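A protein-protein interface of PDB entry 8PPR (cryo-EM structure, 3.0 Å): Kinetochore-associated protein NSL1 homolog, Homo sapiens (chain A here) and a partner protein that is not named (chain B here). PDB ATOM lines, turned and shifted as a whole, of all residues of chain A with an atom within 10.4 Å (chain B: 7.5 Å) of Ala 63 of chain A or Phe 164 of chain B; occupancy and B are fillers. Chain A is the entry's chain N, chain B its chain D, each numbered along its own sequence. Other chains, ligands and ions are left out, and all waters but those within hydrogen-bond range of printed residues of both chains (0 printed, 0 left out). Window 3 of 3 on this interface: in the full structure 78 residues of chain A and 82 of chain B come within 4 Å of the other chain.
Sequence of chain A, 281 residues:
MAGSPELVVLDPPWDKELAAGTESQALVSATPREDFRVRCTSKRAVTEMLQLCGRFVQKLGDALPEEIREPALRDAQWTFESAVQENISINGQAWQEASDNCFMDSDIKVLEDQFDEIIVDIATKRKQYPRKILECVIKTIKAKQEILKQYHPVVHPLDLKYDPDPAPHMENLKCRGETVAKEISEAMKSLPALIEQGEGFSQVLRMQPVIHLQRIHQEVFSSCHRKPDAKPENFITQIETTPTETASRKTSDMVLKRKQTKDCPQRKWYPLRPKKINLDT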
ATOM      1  N   VAL A  57      33.234   0.632  25.730  1.00  0.00           N
ATOM      2  CA  VAL A  57      32.437   0.329  24.547  1.00  0.00           C
ATOM      3  C   VAL A  57      31.393  -0.735  24.867  1.00  0.00           C
ATOM      4  O   VAL A  57      30.253  -0.671  24.391  1.00  0.00           O
ATOM      5  CB  VAL A  57      33.354  -0.102  23.386  1.00  0.00           C
ATOM      6  CG1 VAL A  57      32.533  -0.476  22.161  1.00  0.00           C
ATOM      7  CG2 VAL A  57      34.349   1.002  23.058  1.00  0.00           C
ATOM      8  N   GLN A  58      31.767  -1.730  25.677  1.00  0.00           N
ATOM      9  CA  GLN A  58      30.853  -2.825  25.998  1.00  0.00           C
ATOM     10  C   GLN A  58      29.623  -2.343  26.761  1.00  0.00           C
ATOM     11  O   GLN A  58      28.567  -2.984  26.702  1.00  0.00           O
ATOM     12  CB  GLN A  58      31.591  -3.895  26.804  1.00  0.00           C
ATOM     13  CG  GLN A  58      31.150  -5.320  26.517  1.00  0.00           C
ATOM     14  CD  GLN A  58      29.928  -5.722  27.319  1.00  0.00           C
ATOM     15  OE1 GLN A  58      29.650  -5.151  28.373  1.00  0.00           O
ATOM     16  NE2 GLN A  58      29.198  -6.716  26.829  1.00  0.00           N
ATOM     17  N   LYS A  59      29.739  -1.227  27.485  1.00  0.00           N
ATOM     18  CA  LYS A  59      28.616  -0.699  28.249  1.00  0.00           C
ATOM     19  C   LYS A  59      27.453  -0.282  27.360  1.00  0.00           C
ATOM     20  O   LYS A  59      26.331  -0.136  27.855  1.00  0.00           O
ATOM     21  CB  LYS A  59      29.070   0.492  29.097  1.00  0.00           C
ATOM     22  CG  LYS A  59      29.749   0.108  30.400  1.00  0.00           C
ATOM     23  CD  LYS A  59      30.377   1.318  31.071  1.00  0.00           C
ATOM     24  CE  LYS A  59      29.327   2.343  31.467  1.00  0.00           C
ATOM     25  NZ  LYS A  59      29.938   3.534  32.121  1.00  0.00           N
ATOM     26  N   LEU A  60      27.695  -0.082  26.063  1.00  0.00           N
ATOM     27  CA  LEU A  60      26.618   0.275  25.149  1.00  0.00           C
ATOM     28  C   LEU A  60      25.579  -0.830  25.022  1.00  0.00           C
ATOM     29  O   LEU A  60      24.419  -0.539  24.712  1.00  0.00           O
ATOM     30  CB  LEU A  60      27.182   0.604  23.764  1.00  0.00           C
ATOM     31  CG  LEU A  60      27.702   2.021  23.489  1.00  0.00           C
ATOM     32  CD1 LEU A  60      26.594   3.053  23.653  1.00  0.00           C
ATOM     33  CD2 LEU A  60      28.911   2.366  24.351  1.00  0.00           C
ATOM     34  N   GLY A  61      25.960  -2.082  25.284  1.00  0.00           N
ATOM     35  CA  GLY A  61      25.101  -3.226  25.027  1.00  0.00           C
ATOM     36  C   GLY A  61      23.873  -3.319  25.907  1.00  0.00           C
ATOM     37  O   GLY A  61      22.985  -4.124  25.608  1.00  0.00           O
ATOM     38  N   ASP A  62      23.803  -2.532  26.984  1.00  0.00           N
ATOM     39  CA  ASP A  62      22.615  -2.555  27.832  1.00  0.00           C
ATOM     40  C   ASP A  62      21.384  -2.083  27.069  1.00  0.00           C
ATOM     41  O   ASP A  62      20.292  -2.640  27.230  1.00  0.00           O
ATOM     42  CB  ASP A  62      22.843  -1.701  29.080  1.00  0.00           C
ATOM     43  CG  ASP A  62      23.261  -0.282  28.750  1.00  0.00           C
ATOM     44  OD1 ASP A  62      23.490   0.011  27.557  1.00  0.00           O
ATOM     45  OD2 ASP A  62      23.361   0.542  29.682  1.00  0.00           O
ATOM     46  N   ALA A  63      21.539  -1.053  26.237  1.00  0.00           N
ATOM     47  CA  ALA A  63      20.426  -0.521  25.461  1.00  0.00           C
ATOM     48  C   ALA A  63      20.156  -1.305  24.182  1.00  0.00           C
ATOM     49  O   ALA A  63      19.093  -1.119  23.580  1.00  0.00           O
ATOM     50  CB  ALA A  63      20.682   0.949  25.122  1.00  0.00           C
ATOM     51  N   LEU A  64      21.079  -2.161  23.751  1.00  0.00           N
ATOM     52  CA  LEU A  64      20.838  -2.976  22.568  1.00  0.00           C
ATOM     53  C   LEU A  64      19.741  -4.003  22.844  1.00  0.00           C
ATOM     54  O   LEU A  64      19.645  -4.524  23.960  1.00  0.00           O
ATOM     55  CB  LEU A  64      22.116  -3.693  22.123  1.00  0.00           C
ATOM     56  CG  LEU A  64      23.144  -2.962  21.250  1.00  0.00           C
ATOM     57  CD1 LEU A  64      22.537  -2.611  19.899  1.00  0.00           C
ATOM     58  CD2 LEU A  64      23.706  -1.722  21.924  1.00  0.00           C
ATOM     59  N   PRO A  65      18.903  -4.309  21.857  1.00  0.00           N
ATOM     60  CA  PRO A  65      17.887  -5.350  22.051  1.00  0.00           C
ATOM     61  C   PRO A  65      18.523  -6.715  22.261  1.00  0.00           C
ATOM     62  O   PRO A  65      19.622  -6.997  21.777  1.00  0.00           O
ATOM     63  CB  PRO A  65      17.070  -5.311  20.752  1.00  0.00           C
ATOM     64  CG  PRO A  65      17.467  -4.058  20.047  1.00  0.00           C
ATOM     65  CD  PRO A  65      18.822  -3.672  20.533  1.00  0.00           C
ATOM     66  N   GLU A  66      17.802  -7.568  22.998  1.00  0.00           N
ATOM     67  CA  GLU A  66      18.320  -8.887  23.352  1.00  0.00           C
ATOM     68  C   GLU A  66      18.699  -9.701  22.120  1.00  0.00           C
ATOM     69  O   GLU A  66      19.656 -10.484  22.165  1.00  0.00           O
ATOM     70  CB  GLU A  66      17.283  -9.639  24.192  1.00  0.00           C
ATOM     71  CG  GLU A  66      17.557 -11.126  24.374  1.00  0.00           C
ATOM     72  CD  GLU A  66      18.716 -11.405  25.314  1.00  0.00           C
ATOM     73  OE1 GLU A  66      19.131 -10.480  26.045  1.00  0.00           O
ATOM     74  OE2 GLU A  66      19.212 -12.550  25.323  1.00  0.00           O
ATOM     75  N   GLU A  67      17.976  -9.523  21.013  1.00  0.00           N
ATOM     76  CA  GLU A  67      18.273 -10.284  19.804  1.00  0.00           C
ATOM     77  C   GLU A  67      19.646  -9.932  19.244  1.00  0.00           C
ATOM     78  O   GLU A  67      20.352 -10.801  18.720  1.00  0.00           O
ATOM     79  CB  GLU A  67      17.188 -10.040  18.754  1.00  0.00           C
ATOM     80  CG  GLU A  67      15.775 -10.300  19.249  1.00  0.00           C
ATOM     81  CD  GLU A  67      14.722  -9.929  18.225  1.00  0.00           C
ATOM     82  OE1 GLU A  67      15.084  -9.341  17.183  1.00  0.00           O
ATOM     83  OE2 GLU A  67      13.531 -10.224  18.461  1.00  0.00           O
ATOM     84  N   ILE A  68      20.042  -8.663  19.343  1.00  0.00           N
ATOM     85  CA  ILE A  68      21.287  -8.197  18.743  1.00  0.00           C
ATOM     86  C   ILE A  68      22.202  -7.605  19.808  1.00  0.00           C
ATOM     87  O   ILE A  68      22.968  -6.674  19.533  1.00  0.00           O
ATOM     88  CB  ILE A  68      21.009  -7.172  17.628  1.00  0.00           C
ATOM     89  CG1 ILE A  68      20.086  -6.066  18.142  1.00  0.00           C
ATOM     90  CG2 ILE A  68      20.397  -7.860  16.418  1.00  0.00           C
ATOM     91  CD1 ILE A  68      19.827  -4.966  17.137  1.00  0.00           C
ATOM     92  N   ARG A  69      22.128  -8.136  21.030  1.00  0.00           N
ATOM     93  CA  ARG A  69      22.947  -7.610  22.119  1.00  0.00           C
ATOM     94  C   ARG A  69      24.430  -7.867  21.875  1.00  0.00           C
ATOM     95  O   ARG A  69      25.223  -6.927  21.752  1.00  0.00           O
ATOM     96  CB  ARG A  69      22.508  -8.221  23.452  1.00  0.00           C
ATOM     97  CG  ARG A  69      21.536  -7.364  24.244  1.00  0.00           C
ATOM     98  CD  ARG A  69      21.236  -7.980  25.600  1.00  0.00           C
ATOM     99  NE  ARG A  69      22.405  -7.974  26.473  1.00  0.00           N
ATOM    100  CZ  ARG A  69      22.744  -6.964  27.262  1.00  0.00           C
ATOM    101  NH1 ARG A  69      22.025  -5.855  27.315  1.00  0.00           N
ATOM    102  NH2 ARG A  69      23.834  -7.070  28.018  1.00  0.00           N
ATOM    103  N   GLU A  70      24.823  -9.137  21.801  1.00  0.00           N
ATOM    104  CA  GLU A  70      26.237  -9.490  21.714  1.00  0.00           C
ATOM    105  C   GLU A  70      26.865  -9.299  20.329  1.00  0.00           C
ATOM    106  O   GLU A  70      27.997  -8.803  20.257  1.00  0.00           O
ATOM    107  CB  GLU A  70      26.453 -10.930  22.199  1.00  0.00           C
ATOM    108  CG  GLU A  70      25.575 -11.993  21.558  1.00  0.00           C
ATOM    109  CD  GLU A  70      26.245 -12.663  20.375  1.00  0.00           C
ATOM    110  OE1 GLU A  70      27.477 -12.513  20.224  1.00  0.00           O
ATOM    111  OE2 GLU A  70      25.543 -13.342  19.596  1.00  0.00           O
ATOM    112  N   ALA A  72      26.319  -7.338  17.487  1.00  0.00           N
ATOM    113  CA  ALA A  72      26.565  -5.959  17.081  1.00  0.00           C
ATOM    114  C   ALA A  72      27.584  -5.290  17.996  1.00  0.00           C
ATOM    115  O   ALA A  72      28.468  -4.560  17.536  1.00  0.00           O
ATOM    116  CB  ALA A  72      25.252  -5.177  17.073  1.00  0.00           C
ATOM    117  N   LEU A  73      27.465  -5.526  19.305  1.00  0.00           N
ATOM    118  CA  LEU A  73      28.388  -4.919  20.256  1.00  0.00           C
ATOM    119  C   LEU A  73      29.814  -5.414  20.040  1.00  0.00           C
ATOM    120  O   LEU A  73      30.768  -4.631  20.081  1.00  0.00           O
ATOM    121  CB  LEU A  73      27.927  -5.205  21.686  1.00  0.00           C
ATOM    122  CG  LEU A  73      28.831  -4.691  22.807  1.00  0.00           C
ATOM    123  CD1 LEU A  73      29.039  -3.192  22.680  1.00  0.00           C
ATOM    124  CD2 LEU A  73      28.238  -5.038  24.159  1.00  0.00           C
ATOM    125  N   ALA A  76      31.208  -3.826  16.927  1.00  0.00           N
ATOM    126  CA  ALA A  76      31.610  -2.451  17.209  1.00  0.00           C
ATOM    127  C   ALA A  76      32.913  -2.408  18.000  1.00  0.00           C
ATOM    128  O   ALA A  76      33.757  -1.535  17.772  1.00  0.00           O
ATOM    129  CB  ALA A  76      30.499  -1.722  17.963  1.00  0.00           C
ATOM    130  N   ILE B 146      30.813   4.150  16.631  1.00  0.00           N
ATOM    131  CA  ILE B 146      29.412   4.497  16.862  1.00  0.00           C
ATOM    132  C   ILE B 146      28.706   4.769  15.538  1.00  0.00           C
ATOM    133  O   ILE B 146      27.603   4.268  15.286  1.00  0.00           O
ATOM    134  CB  ILE B 146      29.307   5.701  17.815  1.00  0.00           C
ATOM    135  CG1 ILE B 146      29.661   5.282  19.244  1.00  0.00           C
ATOM    136  CG2 ILE B 146      27.913   6.307  17.760  1.00  0.00           C
ATOM    137  CD1 ILE B 146      28.734   4.235  19.822  1.00  0.00           C
ATOM    138  N   LEU B 149      28.214   1.512  13.573  1.00  0.00           N
ATOM    139  CA  LEU B 149      27.154   0.672  14.118  1.00  0.00           C
ATOM    140  C   LEU B 149      25.776   1.310  13.991  1.00  0.00           C
ATOM    141  O   LEU B 149      24.770   0.595  14.052  1.00  0.00           O
ATOM    142  CB  LEU B 149      27.454   0.351  15.586  1.00  0.00           C
ATOM    143  CG  LEU B 149      26.504  -0.577  16.346  1.00  0.00           C
ATOM    144  CD1 LEU B 149      26.649  -2.006  15.849  1.00  0.00           C
ATOM    145  CD2 LEU B 149      26.756  -0.497  17.843  1.00  0.00           C
ATOM    146  N   GLU B 150      25.711   2.631  13.806  1.00  0.00           N
ATOM    147  CA  GLU B 150      24.416   3.307  13.723  1.00  0.00           C
ATOM    148  C   GLU B 150      23.521   2.780  12.606  1.00  0.00           C
ATOM    149  O   GLU B 150      22.346   2.481  12.882  1.00  0.00           O
ATOM    150  CB  GLU B 150      24.642   4.818  13.592  1.00  0.00           C
ATOM    151  CG  GLU B 150      23.491   5.672  14.092  1.00  0.00           C
ATOM    152  CD  GLU B 150      23.862   7.138  14.190  1.00  0.00           C
ATOM    153  OE1 GLU B 150      25.037   7.474  13.930  1.00  0.00           O
ATOM    154  OE2 GLU B 150      22.978   7.955  14.519  1.00  0.00           O
ATOM    155  N   LEU B 153      22.443  -1.899  12.129  1.00  0.00           N
ATOM    156  CA  LEU B 153      21.333  -2.625  12.734  1.00  0.00           C
ATOM    157  C   LEU B 153      20.009  -1.882  12.604  1.00  0.00           C
ATOM    158  O   LEU B 153      19.086  -2.124  13.388  1.00  0.00           O
ATOM    159  CB  LEU B 153      21.633  -2.927  14.204  1.00  0.00           C
ATOM    160  CG  LEU B 153      22.460  -4.184  14.503  1.00  0.00           C
ATOM    161  CD1 LEU B 153      21.731  -5.429  14.016  1.00  0.00           C
ATOM    162  CD2 LEU B 153      23.860  -4.109  13.908  1.00  0.00           C
ATOM    163  N   GLY B 158      12.700  -2.342  15.652  1.00  0.00           N
ATOM    164  CA  GLY B 158      12.918  -1.570  16.858  1.00  0.00           C
ATOM    165  C   GLY B 158      14.384  -1.240  17.038  1.00  0.00           C
ATOM    166  O   GLY B 158      15.224  -2.143  17.116  1.00  0.00           O
ATOM    167  N   PHE B 159      14.706   0.049  17.114  1.00  0.00           N
ATOM    168  CA  PHE B 159      16.102   0.471  17.197  1.00  0.00           C
ATOM    169  C   PHE B 159      16.123   1.877  17.778  1.00  0.00           C
ATOM    170  O   PHE B 159      15.707   2.828  17.109  1.00  0.00           O
ATOM    171  CB  PHE B 159      16.756   0.425  15.820  1.00  0.00           C
ATOM    172  CG  PHE B 159      18.207   0.800  15.821  1.00  0.00           C
ATOM    173  CD1 PHE B 159      19.164  -0.088  16.281  1.00  0.00           C
ATOM    174  CD2 PHE B 159      18.617   2.039  15.359  1.00  0.00           C
ATOM    175  CE1 PHE B 159      20.502   0.248  16.279  1.00  0.00           C
ATOM    176  CE2 PHE B 159      19.954   2.386  15.356  1.00  0.00           C
ATOM    177  CZ  PHE B 159      20.897   1.489  15.818  1.00  0.00           C
ATOM    178  N   SER B 160      16.607   2.007  19.014  1.00  0.00           N
ATOM    179  CA  SER B 160      16.597   3.284  19.729  1.00  0.00           C
ATOM    180  C   SER B 160      17.792   4.126  19.276  1.00  0.00           C
ATOM    181  O   SER B 160      18.803   4.270  19.965  1.00  0.00           O
ATOM    182  CB  SER B 160      16.607   3.051  21.233  1.00  0.00           C
ATOM    183  OG  SER B 160      16.420   4.266  21.936  1.00  0.00           O
ATOM    184  N   LEU B 161      17.652   4.689  18.074  1.00  0.00           N
ATOM    185  CA  LEU B 161      18.757   5.412  17.454  1.00  0.00           C
ATOM    186  C   LEU B 161      19.033   6.734  18.165  1.00  0.00           C
ATOM    187  O   LEU B 161      20.196   7.098  18.377  1.00  0.00           O
ATOM    188  CB  LEU B 161      18.449   5.629  15.968  1.00  0.00           C
ATOM    189  CG  LEU B 161      19.482   6.202  14.995  1.00  0.00           C
ATOM    190  CD1 LEU B 161      19.184   5.704  13.590  1.00  0.00           C
ATOM    191  CD2 LEU B 161      19.482   7.720  15.010  1.00  0.00           C
ATOM    192  N   GLU B 162      17.980   7.464  18.545  1.00  0.00           N
ATOM    193  CA  GLU B 162      18.172   8.755  19.204  1.00  0.00           C
ATOM    194  C   GLU B 162      18.838   8.593  20.568  1.00  0.00           C
ATOM    195  O   GLU B 162      19.778   9.328  20.900  1.00  0.00           O
ATOM    196  CB  GLU B 162      16.834   9.487  19.333  1.00  0.00           C
ATOM    197  CG  GLU B 162      15.733   8.713  20.050  1.00  0.00           C
ATOM    198  CD  GLU B 162      14.911   7.850  19.113  1.00  0.00           C
ATOM    199  OE1 GLU B 162      15.343   7.639  17.961  1.00  0.00           O
ATOM    200  OE2 GLU B 162      13.830   7.384  19.531  1.00  0.00           O
ATOM    201  N   SER B 163      18.371   7.630  21.368  1.00  0.00           N
ATOM    202  CA  SER B 163      19.025   7.364  22.642  1.00  0.00           C
ATOM    203  C   SER B 163      20.429   6.823  22.432  1.00  0.00           C
ATOM    204  O   SER B 163      21.315   7.070  23.257  1.00  0.00           O
ATOM    205  CB  SER B 163      18.196   6.385  23.473  1.00  0.00           C
ATOM    206  OG  SER B 163      18.395   5.053  23.035  1.00  0.00           O
ATOM    207  N   PHE B 164      20.653   6.098  21.334  1.00  0.00           N
ATOM    208  CA  PHE B 164      21.998   5.638  21.016  1.00  0.00           C
ATOM    209  C   PHE B 164      22.939   6.813  20.794  1.00  0.00           C
ATOM    210  O   PHE B 164      24.056   6.830  21.319  1.00  0.00           O
ATOM    211  CB  PHE B 164      21.968   4.728  19.787  1.00  0.00           C
ATOM    212  CG  PHE B 164      21.723   3.284  20.114  1.00  0.00           C
ATOM    213  CD1 PHE B 164      21.398   2.900  21.402  1.00  0.00           C
ATOM    214  CD2 PHE B 164      21.817   2.311  19.133  1.00  0.00           C
ATOM    215  CE1 PHE B 164      21.171   1.574  21.708  1.00  0.00           C
ATOM    216  CE2 PHE B 164      21.592   0.983  19.434  1.00  0.00           C
ATOM    217  CZ  PHE B 164      21.267   0.615  20.723  1.00  0.00           C
ATOM    218  N   ARG B 165      22.499   7.818  20.030  1.00  0.00           N
ATOM    219  CA  ARG B 165      23.344   8.991  19.819  1.00  0.00           C
ATOM    220  C   ARG B 165      23.544   9.775  21.110  1.00  0.00           C
ATOM    221  O   ARG B 165      24.646  10.270  21.376  1.00  0.00           O
ATOM    222  CB  ARG B 165      22.756   9.896  18.738  1.00  0.00           C
ATOM    223  CG  ARG B 165      22.363   9.188  17.460  1.00  0.00           C
ATOM    224  CD  ARG B 165      21.629  10.136  16.529  1.00  0.00           C
ATOM    225  NE  ARG B 165      20.332  10.534  17.061  1.00  0.00           N
ATOM    226  CZ  ARG B 165      20.071  11.725  17.581  1.00  0.00           C
ATOM    227  NH1 ARG B 165      21.001  12.663  17.658  1.00  0.00           N
ATOM    228  NH2 ARG B 165      18.848  11.982  18.038  1.00  0.00           N
ATOM    229  N   ALA B 166      22.488   9.916  21.915  1.00  0.00           N
ATOM    230  CA  ALA B 166      22.617  10.643  23.176  1.00  0.00           C
ATOM    231  C   ALA B 166      23.624   9.966  24.099  1.00  0.00           C
ATOM    232  O   ALA B 166      24.515  10.622  24.660  1.00  0.00           O
ATOM    233  CB  ALA B 166      21.253  10.761  23.855  1.00  0.00           C
ATOM    234  N   LYS B 167      23.508   8.645  24.255  1.00  0.00           N
ATOM    235  CA  LYS B 167      24.447   7.909  25.090  1.00  0.00           C
ATOM    236  C   LYS B 167      25.846   7.916  24.493  1.00  0.00           C
ATOM    237  O   LYS B 167      26.829   7.952  25.237  1.00  0.00           O
ATOM    238  CB  LYS B 167      23.963   6.474  25.295  1.00  0.00           C
ATOM    239  CG  LYS B 167      24.866   5.648  26.196  1.00  0.00           C
ATOM    240  CD  LYS B 167      24.352   4.230  26.353  1.00  0.00           C
ATOM    241  CE  LYS B 167      25.287   3.408  27.223  1.00  0.00           C
ATOM    242  NZ  LYS B 167      24.817   2.006  27.362  1.00  0.00           N
ATOM    243  N   ALA B 168      25.960   7.885  23.163  1.00  0.00           N
ATOM    244  CA  ALA B 168      27.272   7.956  22.533  1.00  0.00           C
ATOM    245  C   ALA B 168      27.953   9.282  22.833  1.00  0.00           C
ATOM    246  O   ALA B 168      29.146   9.314  23.146  1.00  0.00           O
ATOM    247  CB  ALA B 168      27.143   7.746  21.025  1.00  0.00           C
ATOM    248  N   SER B 169      27.210  10.388  22.757  1.00  0.00           N
ATOM    249  CA  SER B 169      27.789  11.689  23.083  1.00  0.00           C
ATOM    250  C   SER B 169      28.171  11.774  24.558  1.00  0.00           C
ATOM    251  O   SER B 169      29.260  12.258  24.902  1.00  0.00           O
ATOM    252  CB  SER B 169      26.813  12.805  22.714  1.00  0.00           C
ATOM    253  OG  SER B 169      25.602  12.685  23.440  1.00  0.00           O
ATOM    254  N   SER B 170      27.286  11.307  25.445  1.00  0.00           N
ATOM    255  CA  SER B 170      27.586  11.355  26.874  1.00  0.00           C
ATOM    256  C   SER B 170      28.810  10.512  27.209  1.00  0.00           C
ATOM    257  O   SER B 170      29.694  10.950  27.959  1.00  0.00           O
ATOM    258  CB  SER B 170      26.374  10.889  27.680  1.00  0.00           C
ATOM    259  OG  SER B 170      26.709  10.707  29.045  1.00  0.00           O
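OD1 of Asp 62 of chain A lies within salt-bridge range of NZ of Lys 167 of chain B (2.4 Å). The side-chain amino group (NZ) of Lys 167 of chain B is in hydrogen-bond range of the backbone carbonyl oxygen (O) of Lys 59 of chain A (2.7 Å).
Among the printed residues, merely in contact across the chains: Leu 60 of chain A with Lys 167 of chain B, Ala 63 of chain A with Phe 164 of chain B, Ala 72 of chain A with Leu 149 of chain B, Leu 64 of chain A with Phe 164 of chain B, Ala 72 of chain A with Leu 153 of chain B, Ile 68 of chain A with Leu 153 of chain B and Ala 76 of chain A with Leu 149 of chain B.
Phe 164 of chain B touches two residues of chain A. No residue of chain A comes within 4 Å of Ser 160 of chain B. Lys 167 of chain B touches three residues of chain A. No residue of chain A comes within 4 Å of Ala 168 of chain B. Of the printed residues of chain B, Ala 76 of chain A touches Leu 149 (3.9 Å). Printed residues of chain B within 4 Å of Leu 60 of chain A: Lys 167. Printed residues of chain B within 4 Å of Ala 72 of chain A: Leu 149 and Leu 153. Printed residues of chain B within 4 Å of Asp 62 of chain A: Lys 167. The nearest residue of chain A that does not touch Phe 164 of chain B is Leu 60 of chain A (4.9 Å).
Of the 17 printed residues of chain B, 4 touch a printed residue of chain A. Printed residues of chain B that touch a printed residue of chain A: Leu 149, Leu 153, Phe 164 and Lys 167.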
